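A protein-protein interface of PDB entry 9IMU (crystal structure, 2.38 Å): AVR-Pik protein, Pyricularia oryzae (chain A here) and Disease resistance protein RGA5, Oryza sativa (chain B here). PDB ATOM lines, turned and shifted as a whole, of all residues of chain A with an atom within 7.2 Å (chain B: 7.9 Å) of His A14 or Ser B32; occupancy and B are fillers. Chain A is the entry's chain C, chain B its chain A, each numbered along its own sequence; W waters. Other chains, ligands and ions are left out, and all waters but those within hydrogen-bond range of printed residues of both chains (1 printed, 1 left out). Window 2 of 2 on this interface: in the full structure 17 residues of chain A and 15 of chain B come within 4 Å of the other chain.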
ATOM      1  N   PHE A  12      21.723  26.137  -4.451  1.00  0.00           N
ATOM      2  CA  PHE A  12      22.387  27.430  -4.487  1.00  0.00           C
ATOM      3  C   PHE A  12      21.709  28.249  -5.577  1.00  0.00           C
ATOM      4  O   PHE A  12      21.794  27.891  -6.756  1.00  0.00           O
ATOM      5  CB  PHE A  12      23.879  27.261  -4.751  1.00  0.00           C
ATOM      6  CG  PHE A  12      24.552  28.521  -5.124  1.00  0.00           C
ATOM      7  CD1 PHE A  12      24.710  29.530  -4.192  1.00  0.00           C
ATOM      8  CD2 PHE A  12      24.998  28.730  -6.421  1.00  0.00           C
ATOM      9  CE1 PHE A  12      25.322  30.733  -4.543  1.00  0.00           C
ATOM     10  CE2 PHE A  12      25.617  29.926  -6.785  1.00  0.00           C
ATOM     11  CZ  PHE A  12      25.782  30.926  -5.842  1.00  0.00           C
ATOM     12  N   ASP A  13      21.028  29.331  -5.193  1.00  0.00           N
ATOM     13  CA  ASP A  13      20.334  30.185  -6.154  1.00  0.00           C
ATOM     14  C   ASP A  13      21.308  31.187  -6.754  1.00  0.00           C
ATOM     15  O   ASP A  13      21.846  32.043  -6.044  1.00  0.00           O
ATOM     16  CB  ASP A  13      19.181  30.934  -5.500  1.00  0.00           C
ATOM     17  CG  ASP A  13      18.057  30.014  -5.063  1.00  0.00           C
ATOM     18  OD1 ASP A  13      17.608  29.181  -5.878  1.00  0.00           O
ATOM     19  OD2 ASP A  13      17.633  30.123  -3.891  1.00  0.00           O
ATOM     20  N   HIS A  14      21.510  31.096  -8.051  1.00  0.00           N
ATOM     21  CA  HIS A  14      22.461  31.960  -8.729  1.00  0.00           C
ATOM     22  C   HIS A  14      21.947  33.393  -8.733  1.00  0.00           C
ATOM     23  O   HIS A  14      20.763  33.619  -9.014  1.00  0.00           O
ATOM     24  CB  HIS A  14      22.659  31.453 -10.145  1.00  0.00           C
ATOM     25  CG  HIS A  14      22.900  29.977 -10.208  1.00  0.00           C
ATOM     26  ND1 HIS A  14      21.873  29.056 -10.145  1.00  0.00           N
ATOM     27  CD2 HIS A  14      24.042  29.263 -10.352  1.00  0.00           C
ATOM     28  CE1 HIS A  14      22.377  27.834 -10.226  1.00  0.00           C
ATOM     29  NE2 HIS A  14      23.691  27.932 -10.354  1.00  0.00           N
ATOM     30  N   PRO A  15      22.788  34.377  -8.412  1.00  0.00           N
ATOM     31  CA  PRO A  15      22.279  35.746  -8.228  1.00  0.00           C
ATOM     32  C   PRO A  15      21.633  36.351  -9.460  1.00  0.00           C
ATOM     33  O   PRO A  15      20.691  37.150  -9.339  1.00  0.00           O
ATOM     34  CB  PRO A  15      23.525  36.534  -7.813  1.00  0.00           C
ATOM     35  CG  PRO A  15      24.469  35.513  -7.242  1.00  0.00           C
ATOM     36  CD  PRO A  15      24.113  34.162  -7.802  1.00  0.00           C
ATOM     37  N   GLY A  16      22.089  36.037 -10.657  1.00  0.00           N
ATOM     38  CA  GLY A  16      21.453  36.677 -11.796  1.00  0.00           C
ATOM     39  C   GLY A  16      20.049  36.184 -12.125  1.00  0.00           C
ATOM     40  O   GLY A  16      19.254  36.932 -12.674  1.00  0.00           O
ATOM     41  N   ILE A  17      19.733  34.924 -11.836  1.00  0.00           N
ATOM     42  CA  ILE A  17      18.603  34.313 -12.539  1.00  0.00           C
ATOM     43  C   ILE A  17      17.358  34.306 -11.659  1.00  0.00           C
ATOM     44  O   ILE A  17      17.462  34.436 -10.430  1.00  0.00           O
ATOM     45  CB  ILE A  17      18.943  32.891 -13.011  1.00  0.00           C
ATOM     46  CG1 ILE A  17      19.151  31.976 -11.827  1.00  0.00           C
ATOM     47  CG2 ILE A  17      20.241  32.920 -13.841  1.00  0.00           C
ATOM     48  CD1 ILE A  17      19.021  30.511 -12.169  1.00  0.00           C
ATOM     49  N   PRO A  18      16.164  34.169 -12.230  1.00  0.00           N
ATOM     50  CA  PRO A  18      14.967  34.132 -11.386  1.00  0.00           C
ATOM     51  C   PRO A  18      14.958  32.911 -10.481  1.00  0.00           C
ATOM     52  O   PRO A  18      15.384  31.812 -10.854  1.00  0.00           O
ATOM     53  CB  PRO A  18      13.808  34.128 -12.390  1.00  0.00           C
ATOM     54  CG  PRO A  18      14.428  33.847 -13.712  1.00  0.00           C
ATOM     55  CD  PRO A  18      15.828  34.364 -13.649  1.00  0.00           C
ATOM     56  N   VAL A  19      14.506  33.141  -9.257  1.00  0.00           N
ATOM     57  CA  VAL A  19      14.600  32.148  -8.201  1.00  0.00           C
ATOM     58  C   VAL A  19      13.537  31.097  -8.469  1.00  0.00           C
ATOM     59  O   VAL A  19      12.342  31.407  -8.518  1.00  0.00           O
ATOM     60  CB  VAL A  19      14.444  32.800  -6.819  1.00  0.00           C
ATOM     61  CG1 VAL A  19      14.483  31.757  -5.743  1.00  0.00           C
ATOM     62  CG2 VAL A  19      15.542  33.854  -6.622  1.00  0.00           C
ATOM     63  N   PRO A  20      13.919  29.849  -8.656  1.00  0.00           N
ATOM     64  CA  PRO A  20      12.906  28.822  -8.882  1.00  0.00           C
ATOM     65  C   PRO A  20      12.040  28.671  -7.640  1.00  0.00           C
ATOM     66  O   PRO A  20      12.521  28.809  -6.514  1.00  0.00           O
ATOM     67  CB  PRO A  20      13.729  27.570  -9.196  1.00  0.00           C
ATOM     68  CG  PRO A  20      15.125  27.869  -8.664  1.00  0.00           C
ATOM     69  CD  PRO A  20      15.298  29.336  -8.583  1.00  0.00           C
ATOM     70  N   THR A  37      15.731  22.044  -7.156  1.00  0.00           N
ATOM     71  CA  THR A  37      14.818  23.147  -7.352  1.00  0.00           C
ATOM     72  C   THR A  37      14.371  23.154  -8.803  1.00  0.00           C
ATOM     73  O   THR A  37      15.093  22.705  -9.700  1.00  0.00           O
ATOM     74  CB  THR A  37      15.467  24.503  -6.976  1.00  0.00           C
ATOM     75  OG1 THR A  37      16.684  24.664  -7.699  1.00  0.00           O
ATOM     76  CG2 THR A  37      15.811  24.583  -5.504  1.00  0.00           C
ATOM     77  N   TYR A  39      11.376  25.414 -11.625  1.00  0.00           N
ATOM     78  CA  TYR A  39      10.390  26.465 -11.748  1.00  0.00           C
ATOM     79  C   TYR A  39       8.988  25.901 -11.630  1.00  0.00           C
ATOM     80  O   TYR A  39       8.728  24.743 -11.972  1.00  0.00           O
ATOM     81  CB  TYR A  39      10.576  27.193 -13.069  1.00  0.00           C
ATOM     82  CG  TYR A  39      11.849  27.987 -13.025  1.00  0.00           C
ATOM     83  CD1 TYR A  39      11.920  29.162 -12.289  1.00  0.00           C
ATOM     84  CD2 TYR A  39      12.990  27.541 -13.673  1.00  0.00           C
ATOM     85  CE1 TYR A  39      13.094  29.893 -12.222  1.00  0.00           C
ATOM     86  CE2 TYR A  39      14.156  28.258 -13.615  1.00  0.00           C
ATOM     87  CZ  TYR A  39      14.202  29.440 -12.895  1.00  0.00           C
ATOM     88  OH  TYR A  39      15.367  30.153 -12.821  1.00  0.00           O
ATOM     89  N   ARG B   2      18.882  31.005 -21.804  1.00  0.00           N
ATOM     90  CA  ARG B   2      19.636  30.500 -20.666  1.00  0.00           C
ATOM     91  C   ARG B   2      19.014  29.191 -20.193  1.00  0.00           C
ATOM     92  O   ARG B   2      17.797  29.018 -20.230  1.00  0.00           O
ATOM     93  CB  ARG B   2      19.662  31.543 -19.542  1.00  0.00           C
ATOM     94  CG  ARG B   2      20.618  31.194 -18.415  1.00  0.00           C
ATOM     95  CD  ARG B   2      20.970  32.412 -17.546  1.00  0.00           C
ATOM     96  NE  ARG B   2      22.060  33.185 -18.122  1.00  0.00           N
ATOM     97  CZ  ARG B   2      22.036  34.500 -18.294  1.00  0.00           C
ATOM     98  NH1 ARG B   2      23.069  35.104 -18.849  1.00  0.00           N
ATOM     99  NH2 ARG B   2      20.972  35.208 -17.932  1.00  0.00           N
ATOM    100  N   THR B   3      19.862  28.238 -19.809  1.00  0.00           N
ATOM    101  CA  THR B   3      19.398  26.943 -19.332  1.00  0.00           C
ATOM    102  C   THR B   3      20.333  26.489 -18.228  1.00  0.00           C
ATOM    103  O   THR B   3      21.506  26.870 -18.177  1.00  0.00           O
ATOM    104  CB  THR B   3      19.316  25.833 -20.424  1.00  0.00           C
ATOM    105  OG1 THR B   3      20.622  25.365 -20.757  1.00  0.00           O
ATOM    106  CG2 THR B   3      18.684  26.314 -21.689  1.00  0.00           C
ATOM    107  N   LYS B   4      19.790  25.700 -17.324  1.00  0.00           N
ATOM    108  CA  LYS B   4      20.561  25.055 -16.283  1.00  0.00           C
ATOM    109  C   LYS B   4      20.680  23.580 -16.636  1.00  0.00           C
ATOM    110  O   LYS B   4      19.703  22.960 -17.077  1.00  0.00           O
ATOM    111  CB  LYS B   4      19.890  25.254 -14.928  1.00  0.00           C
ATOM    112  CG  LYS B   4      20.330  24.267 -13.887  1.00  0.00           C
ATOM    113  CD  LYS B   4      19.734  24.598 -12.536  1.00  0.00           C
ATOM    114  CE  LYS B   4      18.394  23.895 -12.334  1.00  0.00           C
ATOM    115  NZ  LYS B   4      17.815  24.199 -10.975  1.00  0.00           N
ATOM    116  N   ILE B   5      21.881  23.034 -16.486  1.00  0.00           N
ATOM    117  CA  ILE B   5      22.162  21.636 -16.784  1.00  0.00           C
ATOM    118  C   ILE B   5      22.901  21.040 -15.594  1.00  0.00           C
ATOM    119  O   ILE B   5      23.924  21.580 -15.162  1.00  0.00           O
ATOM    120  CB  ILE B   5      23.009  21.469 -18.060  1.00  0.00           C
ATOM    121  CG1 ILE B   5      22.465  22.280 -19.223  1.00  0.00           C
ATOM    122  CG2 ILE B   5      23.085  20.035 -18.451  1.00  0.00           C
ATOM    123  CD1 ILE B   5      23.472  22.392 -20.339  1.00  0.00           C
ATOM    124  N   LEU B  21      35.325  21.346 -13.076  1.00  0.00           N
ATOM    125  CA  LEU B  21      34.821  22.715 -13.042  1.00  0.00           C
ATOM    126  C   LEU B  21      35.421  23.544 -14.165  1.00  0.00           C
ATOM    127  O   LEU B  21      34.705  24.046 -15.042  1.00  0.00           O
ATOM    128  CB  LEU B  21      35.138  23.352 -11.693  1.00  0.00           C
ATOM    129  CG  LEU B  21      34.213  23.085 -10.513  1.00  0.00           C
ATOM    130  CD1 LEU B  21      34.876  23.593  -9.229  1.00  0.00           C
ATOM    131  CD2 LEU B  21      32.831  23.708 -10.725  1.00  0.00           C
ATOM    132  N   ALA B  24      34.149  22.426 -17.493  1.00  0.00           N
ATOM    133  CA  ALA B  24      32.780  22.851 -17.777  1.00  0.00           C
ATOM    134  C   ALA B  24      32.721  24.357 -18.019  1.00  0.00           C
ATOM    135  O   ALA B  24      32.012  24.820 -18.921  1.00  0.00           O
ATOM    136  CB  ALA B  24      31.842  22.440 -16.638  1.00  0.00           C
ATOM    137  N   ALA B  25      33.499  25.133 -17.251  1.00  0.00           N
ATOM    138  CA  ALA B  25      33.500  26.588 -17.356  1.00  0.00           C
ATOM    139  C   ALA B  25      34.244  27.103 -18.580  1.00  0.00           C
ATOM    140  O   ALA B  25      34.052  28.263 -18.962  1.00  0.00           O
ATOM    141  CB  ALA B  25      34.122  27.210 -16.104  1.00  0.00           C
ATOM    142  N   GLY B  29      29.499  29.865 -23.787  1.00  0.00           N
ATOM    143  CA  GLY B  29      28.162  30.178 -23.350  1.00  0.00           C
ATOM    144  C   GLY B  29      27.886  29.946 -21.883  1.00  0.00           C
ATOM    145  O   GLY B  29      26.793  30.284 -21.424  1.00  0.00           O
ATOM    146  N   VAL B  30      28.839  29.400 -21.129  1.00  0.00           N
ATOM    147  CA  VAL B  30      28.593  29.103 -19.726  1.00  0.00           C
ATOM    148  C   VAL B  30      28.639  30.388 -18.908  1.00  0.00           C
ATOM    149  O   VAL B  30      29.460  31.276 -19.156  1.00  0.00           O
ATOM    150  CB  VAL B  30      29.609  28.067 -19.219  1.00  0.00           C
ATOM    151  CG1 VAL B  30      29.463  27.859 -17.725  1.00  0.00           C
ATOM    152  CG2 VAL B  30      29.401  26.751 -19.941  1.00  0.00           C
ATOM    153  N   ASP B  31      27.748  30.492 -17.925  1.00  0.00           N
ATOM    154  CA  ASP B  31      27.743  31.620 -16.999  1.00  0.00           C
ATOM    155  C   ASP B  31      28.346  31.263 -15.646  1.00  0.00           C
ATOM    156  O   ASP B  31      29.134  32.039 -15.100  1.00  0.00           O
ATOM    157  CB  ASP B  31      26.316  32.133 -16.798  1.00  0.00           C
ATOM    158  CG  ASP B  31      25.754  32.766 -18.046  1.00  0.00           C
ATOM    159  OD1 ASP B  31      26.488  33.522 -18.688  1.00  0.00           O
ATOM    160  OD2 ASP B  31      24.581  32.522 -18.386  1.00  0.00           O
ATOM    161  N   SER B  32      27.980  30.104 -15.094  1.00  0.00           N
ATOM    162  CA  SER B  32      28.513  29.635 -13.823  1.00  0.00           C
ATOM    163  C   SER B  32      28.652  28.118 -13.841  1.00  0.00           C
ATOM    164  O   SER B  32      27.969  27.408 -14.586  1.00  0.00           O
ATOM    165  CB  SER B  32      27.624  30.029 -12.631  1.00  0.00           C
ATOM    166  OG  SER B  32      26.287  29.589 -12.821  1.00  0.00           O
ATOM    167  N   VAL B  33      29.545  27.633 -12.988  1.00  0.00           N
ATOM    168  CA  VAL B  33      29.673  26.214 -12.689  1.00  0.00           C
ATOM    169  C   VAL B  33      29.762  26.072 -11.178  1.00  0.00           C
ATOM    170  O   VAL B  33      30.560  26.754 -10.530  1.00  0.00           O
ATOM    171  CB  VAL B  33      30.895  25.589 -13.387  1.00  0.00           C
ATOM    172  CG1 VAL B  33      30.726  25.668 -14.870  1.00  0.00           C
ATOM    173  CG2 VAL B  33      32.171  26.362 -13.020  1.00  0.00           C
ATOM    174  N   GLU B  34      28.911  25.228 -10.617  1.00  0.00           N
ATOM    175  CA  GLU B  34      28.932  24.917  -9.202  1.00  0.00           C
ATOM    176  C   GLU B  34      28.865  23.406  -9.048  1.00  0.00           C
ATOM    177  O   GLU B  34      28.263  22.706  -9.865  1.00  0.00           O
ATOM    178  CB  GLU B  34      27.771  25.598  -8.453  1.00  0.00           C
ATOM    179  CG  GLU B  34      27.848  25.496  -6.929  1.00  0.00           C
ATOM    180  CD  GLU B  34      29.069  26.216  -6.324  1.00  0.00           C
ATOM    181  OE1 GLU B  34      30.171  25.614  -6.319  1.00  0.00           O
ATOM    182  OE2 GLU B  34      28.937  27.370  -5.837  1.00  0.00           O
ATOM    183  N   ILE B  35      29.524  22.908  -8.014  1.00  0.00           N
ATOM    184  CA  ILE B  35      29.436  21.511  -7.629  1.00  0.00           C
ATOM    185  C   ILE B  35      28.505  21.404  -6.438  1.00  0.00           C
ATOM    186  O   ILE B  35      28.627  22.167  -5.475  1.00  0.00           O
ATOM    187  CB  ILE B  35      30.819  20.928  -7.306  1.00  0.00           C
ATOM    188  CG1 ILE B  35      31.647  20.879  -8.577  1.00  0.00           C
ATOM    189  CG2 ILE B  35      30.684  19.548  -6.705  1.00  0.00           C
ATOM    190  CD1 ILE B  35      33.054  20.590  -8.335  1.00  0.00           C
ATOM    191  N   THR B  36      27.553  20.482  -6.523  1.00  0.00           N
ATOM    192  CA  THR B  36      26.604  20.233  -5.454  1.00  0.00           C
ATOM    193  C   THR B  36      26.474  18.727  -5.269  1.00  0.00           C
ATOM    194  O   THR B  36      27.128  17.931  -5.956  1.00  0.00           O
ATOM    195  CB  THR B  36      25.233  20.858  -5.750  1.00  0.00           C
ATOM    196  OG1 THR B  36      24.664  20.221  -6.901  1.00  0.00           O
ATOM    197  CG2 THR B  36      25.342  22.370  -5.984  1.00  0.00           C
ATOM    198  N   LEU B  43      27.989  18.500 -11.250  1.00  0.00           N
ATOM    199  CA  LEU B  43      28.284  19.802 -11.829  1.00  0.00           C
ATOM    200  C   LEU B  43      26.972  20.458 -12.228  1.00  0.00           C
ATOM    201  O   LEU B  43      26.178  19.858 -12.960  1.00  0.00           O
ATOM    202  CB  LEU B  43      29.164  19.682 -13.067  1.00  0.00           C
ATOM    203  CG  LEU B  43      30.670  19.631 -12.929  1.00  0.00           C
ATOM    204  CD1 LEU B  43      31.251  19.611 -14.327  1.00  0.00           C
ATOM    205  CD2 LEU B  43      31.150  20.841 -12.157  1.00  0.00           C
ATOM    206  N   VAL B  44      26.745  21.673 -11.743  1.00  0.00           N
ATOM    207  CA  VAL B  44      25.634  22.500 -12.189  1.00  0.00           C
ATOM    208  C   VAL B  44      26.199  23.535 -13.148  1.00  0.00           C
ATOM    209  O   VAL B  44      27.098  24.303 -12.790  1.00  0.00           O
ATOM    210  CB  VAL B  44      24.915  23.173 -11.012  1.00  0.00           C
ATOM    211  CG1 VAL B  44      23.632  23.841 -11.497  1.00  0.00           C
ATOM    212  CG2 VAL B  44      24.620  22.165  -9.928  1.00  0.00           C
ATOM    213  N   VAL B  45      25.678  23.558 -14.369  1.00  0.00           N
ATOM    214  CA  VAL B  45      26.167  24.446 -15.415  1.00  0.00           C
ATOM    215  C   VAL B  45      25.011  25.308 -15.897  1.00  0.00           C
ATOM    216  O   VAL B  45      23.939  24.790 -16.228  1.00  0.00           O
ATOM    217  CB  VAL B  45      26.789  23.651 -16.577  1.00  0.00           C
ATOM    218  CG1 VAL B  45      27.384  24.603 -17.598  1.00  0.00           C
ATOM    219  CG2 VAL B  45      27.851  22.704 -16.038  1.00  0.00           C
ATOM    220  N   VAL B  46      25.234  26.612 -15.952  1.00  0.00           N
ATOM    221  CA  VAL B  46      24.232  27.578 -16.372  1.00  0.00           C
ATOM    222  C   VAL B  46      24.816  28.395 -17.504  1.00  0.00           C
ATOM    223  O   VAL B  46      25.915  28.942 -17.370  1.00  0.00           O
ATOM    224  CB  VAL B  46      23.829  28.496 -15.209  1.00  0.00           C
ATOM    225  CG1 VAL B  46      22.799  29.527 -15.644  1.00  0.00           C
ATOM    226  CG2 VAL B  46      23.288  27.661 -14.083  1.00  0.00           C
ATOM    227  N   GLY B  47      24.080  28.508 -18.598  1.00  0.00           N
ATOM    228  CA  GLY B  47      24.478  29.426 -19.652  1.00  0.00           C
ATOM    229  C   GLY B  47      23.464  29.359 -20.762  1.00  0.00           C
ATOM    230  O   GLY B  47      22.462  28.651 -20.668  1.00  0.00           O
ATOM    231  N   ILE B  50      24.203  26.233 -24.734  1.00  0.00           N
ATOM    232  CA  ILE B  50      24.980  25.021 -24.480  1.00  0.00           C
ATOM    233  C   ILE B  50      24.283  23.808 -25.074  1.00  0.00           C
ATOM    234  O   ILE B  50      23.079  23.601 -24.872  1.00  0.00           O
ATOM    235  CB  ILE B  50      25.208  24.814 -22.977  1.00  0.00           C
ATOM    236  CG1 ILE B  50      25.883  26.032 -22.368  1.00  0.00           C
ATOM    237  CG2 ILE B  50      26.030  23.556 -22.740  1.00  0.00           C
ATOM    238  CD1 ILE B  50      25.332  26.358 -21.023  1.00  0.00           C
ATOM    239  N   VAL B  74      15.755  28.285 -18.274  1.00  0.00           N
ATOM    240  CA  VAL B  74      15.430  29.282 -17.263  1.00  0.00           C
ATOM    241  C   VAL B  74      14.133  29.991 -17.643  1.00  0.00           C
ATOM    242  O   VAL B  74      14.024  30.568 -18.727  1.00  0.00           O
ATOM    243  CB  VAL B  74      16.577  30.275 -17.111  1.00  0.00           C
ATOM    244  CG1 VAL B  74      16.125  31.452 -16.234  1.00  0.00           C
ATOM    245  CG2 VAL B  74      17.792  29.528 -16.537  1.00  0.00           C
HETATM  246  O   HOH W   1      18.442  21.545  -9.179  1.00  0.00           O
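O of Thr A37 sits at hydrogen-bond distance from NZ of Lys B4.
The backbone carbonyl oxygen of Arg B2 lies within hydrogen-bond range of the backbone NH of Val B74, 2.9 Å away.
N of Asp B31 is in hydrogen-bond range of O of Val B46, 2.5 Å away.
The backbone carbonyl oxygen (O) of Ser B32 lies within hydrogen-bond range of the backbone NH (N) of Val B46 (3.2 Å).
NE of Arg B2 is in salt-bridge range of OD2 of Asp B31 (2.6 Å).
The backbone carbonyl oxygen (O) of Pro A18 sits at hydrogen-bond distance from the side-chain hydroxyl (OH) of Tyr A39 (2.6 Å).
Among the printed residues, merely in contact across the chains: His A14 with Ser B32 (3.4 Å), His A14 with Val B46 (3.8 Å), Ile A17 with Arg B2 (3.8 Å), Pro A18 with Val B74 (3.9 Å) and Tyr A39 with Val B74 (3.7 Å).
Of the printed residues of chain B, His A14 touches Ser B32 and Val B46.
No residue of chain B comes within 4 Å of Pro A15.
Of the printed residues of chain A, Arg B2 touches Ile A17.
Of the printed residues of chain A, Val B46 touches His A14.
Of the printed residues of chain B, Pro A18 touches Val B74.
Of the printed residues of chain B, Thr A37 touches Lys B4 (3.4 Å).
Printed residues of chain B within 4 Å of Tyr A39: Val B74 (3.7 Å).
The nearest residue of chain B that does not touch His A14 is Val B44 (4.2 Å).
The nearest residue of chain A that does not touch Ser B32 is Phe A12 (6.1 Å).
The nearest printed residue of chain B that does not touch Tyr A39 is Lys B4 (6.1 Å).
Of the 11 printed residues of chain A, 5 touch a printed residue of chain B.
Printed residues of chain A that touch a printed residue of chain B: His A14, Ile A17, Pro A18, Thr A37 and Tyr A39.
Hydrophobic or aromatic side chains of chain A within 4 Å of the printed part of chain B: His A14, Ile A17, Pro A18 and Tyr A39.
Hydrophobic or aromatic side chains of chain B that line the printed part of chain A: Val B46 and Val B74.
Among the printed residues, 6 pairs touch across the chains.
Among the printed residues, no Asp or Glu carboxylate lies within 4 Å of a Lys or Arg side-chain nitrogen of the other chain.
Water W1 bridges the side-chain amino group (NZ) of Lys B4 and the backbone NH (N) of Thr A37.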
